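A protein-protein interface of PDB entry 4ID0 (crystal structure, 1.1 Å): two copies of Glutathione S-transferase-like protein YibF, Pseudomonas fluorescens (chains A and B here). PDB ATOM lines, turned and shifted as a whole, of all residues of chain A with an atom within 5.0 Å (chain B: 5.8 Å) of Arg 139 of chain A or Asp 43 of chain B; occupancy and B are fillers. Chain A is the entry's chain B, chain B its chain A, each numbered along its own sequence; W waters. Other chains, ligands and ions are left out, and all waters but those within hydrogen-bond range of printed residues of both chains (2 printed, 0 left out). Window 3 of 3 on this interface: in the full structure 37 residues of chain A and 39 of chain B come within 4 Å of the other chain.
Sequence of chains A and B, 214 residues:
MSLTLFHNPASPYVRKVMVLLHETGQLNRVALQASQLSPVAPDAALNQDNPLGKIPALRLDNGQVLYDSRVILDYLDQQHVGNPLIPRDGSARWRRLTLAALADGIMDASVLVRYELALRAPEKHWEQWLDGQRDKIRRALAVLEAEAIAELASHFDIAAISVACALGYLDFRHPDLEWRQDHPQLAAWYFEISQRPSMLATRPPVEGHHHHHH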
ATOM      1  N   ASP A 135      20.107  20.862  16.627  1.00  0.00           N
ATOM      2  CA  ASP A 135      20.400  21.961  17.530  1.00  0.00           C
ATOM      3  C   ASP A 135      19.285  22.201  18.543  1.00  0.00           C
ATOM      4  O   ASP A 135      19.590  22.542  19.697  1.00  0.00           O
ATOM      5  CB  ASP A 135      20.726  23.220  16.753  1.00  0.00           C
ATOM      6  CG  ASP A 135      22.102  23.163  16.111  1.00  0.00           C
ATOM      7  OD1 ASP A 135      22.934  22.363  16.611  1.00  0.00           O
ATOM      8  OD2 ASP A 135      22.339  23.895  15.128  1.00  0.00           O
ATOM      9  N   LYS A 136      18.042  22.026  18.140  1.00  0.00           N
ATOM     10  CA  LYS A 136      16.953  22.086  19.106  1.00  0.00           C
ATOM     11  C   LYS A 136      17.113  20.999  20.168  1.00  0.00           C
ATOM     12  O   LYS A 136      16.834  21.239  21.355  1.00  0.00           O
ATOM     13  CB  LYS A 136      15.596  21.930  18.409  1.00  0.00           C
ATOM     14  CG  LYS A 136      15.193  23.144  17.586  1.00  0.00           C
ATOM     15  CD  LYS A 136      13.937  22.914  16.733  1.00  0.00           C
ATOM     16  CE  LYS A 136      13.473  24.225  16.092  1.00  0.00           C
ATOM     17  NZ  LYS A 136      12.285  23.951  15.193  1.00  0.00           N
ATOM     18  N   ILE A 137      17.534  19.799  19.787  1.00  0.00           N
ATOM     19  CA  ILE A 137      17.791  18.750  20.759  1.00  0.00           C
ATOM     20  C   ILE A 137      18.945  19.178  21.661  1.00  0.00           C
ATOM     21  O   ILE A 137      18.842  19.060  22.894  1.00  0.00           O
ATOM     22  CB  ILE A 137      18.126  17.435  20.051  1.00  0.00           C
ATOM     23  CG1 ILE A 137      16.879  16.886  19.330  1.00  0.00           C
ATOM     24  CG2 ILE A 137      18.667  16.418  21.064  1.00  0.00           C
ATOM     25  CD1 ILE A 137      17.171  15.795  18.337  1.00  0.00           C
ATOM     26  N   ARG A 138      20.046  19.685  21.095  1.00  0.00           N
ATOM     27  CA  ARG A 138      21.201  20.082  21.896  1.00  0.00           C
ATOM     28  C   ARG A 138      20.864  21.172  22.873  1.00  0.00           C
ATOM     29  O   ARG A 138      21.322  21.147  24.029  1.00  0.00           O
ATOM     30  CB  ARG A 138      22.404  20.475  21.027  1.00  0.00           C
ATOM     31  CG  ARG A 138      22.985  19.326  20.243  1.00  0.00           C
ATOM     32  CD  ARG A 138      24.088  19.811  19.319  1.00  0.00           C
ATOM     33  NE  ARG A 138      24.654  18.707  18.525  1.00  0.00           N
ATOM     34  CZ  ARG A 138      24.603  18.677  17.188  1.00  0.00           C
ATOM     35  NH1 ARG A 138      23.986  19.656  16.519  1.00  0.00           N
ATOM     36  NH2 ARG A 138      25.129  17.663  16.503  1.00  0.00           N
ATOM     37  N   ARG A 139      20.061  22.159  22.460  1.00  0.00           N
ATOM     38  CA  ARG A 139      19.705  23.222  23.401  1.00  0.00           C
ATOM     39  C   ARG A 139      18.890  22.652  24.557  1.00  0.00           C
ATOM     40  O   ARG A 139      19.041  23.079  25.703  1.00  0.00           O
ATOM     41  CB  ARG A 139      18.953  24.331  22.676  1.00  0.00           C
ATOM     42  CG  ARG A 139      19.901  25.083  21.750  1.00  0.00           C
ATOM     43  CD  ARG A 139      19.242  26.212  21.058  1.00  0.00           C
ATOM     44  NE  ARG A 139      20.185  26.875  20.137  1.00  0.00           N
ATOM     45  CZ  ARG A 139      20.082  28.136  19.770  1.00  0.00           C
ATOM     46  NH1 ARG A 139      19.088  28.878  20.249  1.00  0.00           N
ATOM     47  NH2 ARG A 139      20.974  28.657  18.923  1.00  0.00           N
ATOM     48  N   ALA A 140      17.967  21.725  24.272  1.00  0.00           N
ATOM     49  CA  ALA A 140      17.174  21.103  25.321  1.00  0.00           C
ATOM     50  C   ALA A 140      18.060  20.267  26.260  1.00  0.00           C
ATOM     51  O   ALA A 140      17.825  20.276  27.482  1.00  0.00           O
ATOM     52  CB  ALA A 140      16.048  20.296  24.706  1.00  0.00           C
ATOM     53  N   LEU A 141      19.036  19.576  25.705  1.00  0.00           N
ATOM     54  CA  LEU A 141      19.978  18.832  26.546  1.00  0.00           C
ATOM     55  C   LEU A 141      20.741  19.750  27.520  1.00  0.00           C
ATOM     56  O   LEU A 141      21.033  19.360  28.628  1.00  0.00           O
ATOM     57  CB  LEU A 141      20.971  18.039  25.692  1.00  0.00           C
ATOM     58  CG  LEU A 141      20.386  16.823  24.912  1.00  0.00           C
ATOM     59  CD1 LEU A 141      21.371  16.363  23.870  1.00  0.00           C
ATOM     60  CD2 LEU A 141      19.953  15.712  25.863  1.00  0.00           C
ATOM     61  N   ALA A 142      21.075  20.956  27.074  1.00  0.00           N
ATOM     62  CA  ALA A 142      21.757  21.882  27.956  1.00  0.00           C
ATOM     63  C   ALA A 142      20.904  22.239  29.147  1.00  0.00           C
ATOM     64  O   ALA A 142      21.395  22.305  30.281  1.00  0.00           O
ATOM     65  CB  ALA A 142      22.182  23.114  27.199  1.00  0.00           C
ATOM     66  N   VAL A 143      19.612  22.493  28.912  1.00  0.00           N
ATOM     67  CA  VAL A 143      18.719  22.780  30.016  1.00  0.00           C
ATOM     68  C   VAL A 143      18.626  21.542  30.924  1.00  0.00           C
ATOM     69  O   VAL A 143      18.685  21.652  32.143  1.00  0.00           O
ATOM     70  CB  VAL A 143      17.322  23.214  29.498  1.00  0.00           C
ATOM     71  CG1 VAL A 143      16.281  23.186  30.617  1.00  0.00           C
ATOM     72  CG2 VAL A 143      17.446  24.570  28.811  1.00  0.00           C
ATOM     73  N   GLN B  36       9.547  35.199  17.822  1.00  0.00           N
ATOM     74  CA  GLN B  36       9.686  34.747  16.439  1.00  0.00           C
ATOM     75  C   GLN B  36       9.708  33.237  16.311  1.00  0.00           C
ATOM     76  O   GLN B  36      10.545  32.572  16.912  1.00  0.00           O
ATOM     77  CB  GLN B  36      10.956  35.341  15.812  1.00  0.00           C
ATOM     78  CG  GLN B  36      11.181  34.998  14.349  1.00  0.00           C
ATOM     79  CD  GLN B  36      12.288  35.830  13.752  1.00  0.00           C
ATOM     80  OE1 GLN B  36      12.069  36.979  13.341  1.00  0.00           O
ATOM     81  NE2 GLN B  36      13.495  35.274  13.723  1.00  0.00           N
ATOM     82  N   SER B  38      10.612  29.671  14.951  1.00  0.00           N
ATOM     83  CA  SER B  38      11.895  29.123  14.505  1.00  0.00           C
ATOM     84  C   SER B  38      11.701  27.769  13.824  1.00  0.00           C
ATOM     85  O   SER B  38      11.918  26.694  14.380  1.00  0.00           O
ATOM     86  CB  SER B  38      12.830  29.006  15.700  1.00  0.00           C
ATOM     87  OG  SER B  38      13.004  30.301  16.254  1.00  0.00           O
ATOM     88  N   ALA B  41      16.324  26.667  11.913  1.00  0.00           N
ATOM     89  CA  ALA B  41      17.351  26.871  12.971  1.00  0.00           C
ATOM     90  C   ALA B  41      16.690  27.543  14.179  1.00  0.00           C
ATOM     91  O   ALA B  41      15.864  28.472  14.007  1.00  0.00           O
ATOM     92  CB  ALA B  41      18.462  27.746  12.445  1.00  0.00           C
ATOM     93  N   PRO B  42      17.022  27.120  15.423  1.00  0.00           N
ATOM     94  CA  PRO B  42      16.557  27.883  16.577  1.00  0.00           C
ATOM     95  C   PRO B  42      17.010  29.339  16.464  1.00  0.00           C
ATOM     96  O   PRO B  42      18.051  29.688  15.916  1.00  0.00           O
ATOM     97  CB  PRO B  42      17.313  27.260  17.751  1.00  0.00           C
ATOM     98  CG  PRO B  42      17.866  25.991  17.297  1.00  0.00           C
ATOM     99  CD  PRO B  42      17.900  25.993  15.791  1.00  0.00           C
ATOM    100  N   ASP B  43      16.191  30.231  17.002  1.00  0.00           N
ATOM    101  CA  ASP B  43      16.532  31.680  16.986  1.00  0.00           C
ATOM    102  C   ASP B  43      17.825  31.939  17.723  1.00  0.00           C
ATOM    103  O   ASP B  43      18.036  31.467  18.851  1.00  0.00           O
ATOM    104  CB  ASP B  43      15.369  32.468  17.622  1.00  0.00           C
ATOM    105  CG  ASP B  43      15.403  33.980  17.346  1.00  0.00           C
ATOM    106  OD1 ASP B  43      16.437  34.587  17.150  1.00  0.00           O
ATOM    107  OD2 ASP B  43      14.281  34.557  17.448  1.00  0.00           O
ATOM    108  N   ALA B  44      18.682  32.724  17.109  1.00  0.00           N
ATOM    109  CA  ALA B  44      19.945  33.144  17.719  1.00  0.00           C
ATOM    110  C   ALA B  44      19.761  34.198  18.814  1.00  0.00           C
ATOM    111  O   ALA B  44      20.697  34.401  19.601  1.00  0.00           O
ATOM    112  CB  ALA B  44      20.874  33.679  16.643  1.00  0.00           C
ATOM    113  N   ALA B  45      18.593  34.844  18.853  1.00  0.00           N
ATOM    114  CA  ALA B  45      18.346  35.857  19.888  1.00  0.00           C
ATOM    115  C   ALA B  45      17.541  35.159  20.989  1.00  0.00           C
ATOM    116  O   ALA B  45      16.408  34.794  20.792  1.00  0.00           O
ATOM    117  CB  ALA B  45      17.565  37.043  19.318  1.00  0.00           C
ATOM    118  N   LEU B  46      18.160  34.931  22.126  1.00  0.00           N
ATOM    119  CA  LEU B  46      17.438  34.329  23.244  1.00  0.00           C
ATOM    120  C   LEU B  46      16.904  35.348  24.225  1.00  0.00           C
ATOM    121  O   LEU B  46      17.572  36.332  24.523  1.00  0.00           O
ATOM    122  CB  LEU B  46      18.356  33.403  24.018  1.00  0.00           C
ATOM    123  CG  LEU B  46      19.084  32.359  23.187  1.00  0.00           C
ATOM    124  CD1 LEU B  46      19.980  31.505  24.037  1.00  0.00           C
ATOM    125  CD2 LEU B  46      18.037  31.496  22.471  1.00  0.00           C
ATOM    126  N   PRO B  51      15.117  29.935  27.204  1.00  0.00           N
ATOM    127  CA  PRO B  51      16.297  29.568  26.418  1.00  0.00           C
ATOM    128  C   PRO B  51      16.006  28.597  25.286  1.00  0.00           C
ATOM    129  O   PRO B  51      16.813  28.529  24.337  1.00  0.00           O
ATOM    130  CB  PRO B  51      17.214  28.889  27.445  1.00  0.00           C
ATOM    131  CG  PRO B  51      16.282  28.446  28.544  1.00  0.00           C
ATOM    132  CD  PRO B  51      15.246  29.527  28.615  1.00  0.00           C
ATOM    133  N   LEU B  52      14.893  27.876  25.341  1.00  0.00           N
ATOM    134  CA  LEU B  52      14.565  26.937  24.298  1.00  0.00           C
ATOM    135  C   LEU B  52      13.642  27.592  23.247  1.00  0.00           C
ATOM    136  O   LEU B  52      13.235  26.944  22.303  1.00  0.00           O
ATOM    137  CB  LEU B  52      13.898  25.685  24.880  1.00  0.00           C
ATOM    138  CG  LEU B  52      14.839  24.977  25.879  1.00  0.00           C
ATOM    139  CD1 LEU B  52      14.162  23.635  26.291  1.00  0.00           C
ATOM    140  CD2 LEU B  52      16.223  24.764  25.315  1.00  0.00           C
HETATM  141  O   HOH W   1      20.245  31.340  20.235  1.00  0.00           O
HETATM  142  O   HOH W   2      16.749  28.129  21.677  1.00  0.00           O
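Water W1 lies within hydrogen-bond range of O of Asp 43 of chain B (2.6 Å), NH1 of Arg 139 of chain A (2.7 Å) and O of Ala 44 of chain B (3.2 Å). Water W2 bridges O of Pro 51 of chain B (2.7 Å) and NH1 of Arg 139 of chain A (2.8 Å).
O of Ser 38 of chain B sits at hydrogen-bond distance from NZ of Lys 136 of chain A (2.9 Å). The guanidinium group (NH1) of Arg 139 of chain A lies within hydrogen-bond range of the backbone carbonyl oxygen (O) of Asp 43 of chain B (3.1 Å).
The side-chain hydroxyl (OG) of Ser 38 of chain B sits at hydrogen-bond distance from the backbone carbonyl oxygen (O) of Gln 36 of chain B (3.4 Å). The side-chain hydroxyl (OG) of Ser 38 of chain B lies within hydrogen-bond range of the backbone NH (N) of Asp 43 of chain B, at 3.3 Å. The side-chain carboxylate (OD1) of Asp 43 of chain B sits at hydrogen-bond distance from the backbone NH (N) of Ala 45 of chain B (2.8 Å).
No position is printed for both chains. Of the 8 pairs that touch across the chains among the printed residues, none has its exchanged pair printed and touching as well.
Hydrophobic or aromatic side chains of chain B within 4 Å of the printed part of chain A: Pro 42, Leu 46 and Leu 52. Of the 9 printed residues of chain A, 4 touch a printed residue of chain B. Hydrophobic or aromatic side chains of chain A that line the printed part of chain B: Val 143. Among the printed residues, 8 pairs touch across the chains.
Of chain B, only Pro 42, Asp 43, Leu 46 and Leu 52 come within 4 Å of Arg 139 of chain A. Of the printed residues of chain A, Asp 43 of chain B touches Arg 139. Of the printed residues of chain B, Val 143 of chain A touches Leu 52. Of the printed residues of chain A, Pro 42 of chain B touches Lys 136 (3.9 Å) and Arg 139 (3.5 Å).
Among the printed residues, pairs that only touch across the chains: Arg 139 of chain A with Leu 52 of chain B (3.3 Å), Arg 139 of chain A with Pro 42 of chain B (3.5 Å), Arg 139 of chain A with Leu 46 of chain B (3.6 Å), Ala 140 of chain A with Leu 52 of chain B (3.7 Å), Val 143 of chain A with Leu 52 of chain B (3.7 Å) and Lys 136 of chain A with Pro 42 of chain B (3.9 Å).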
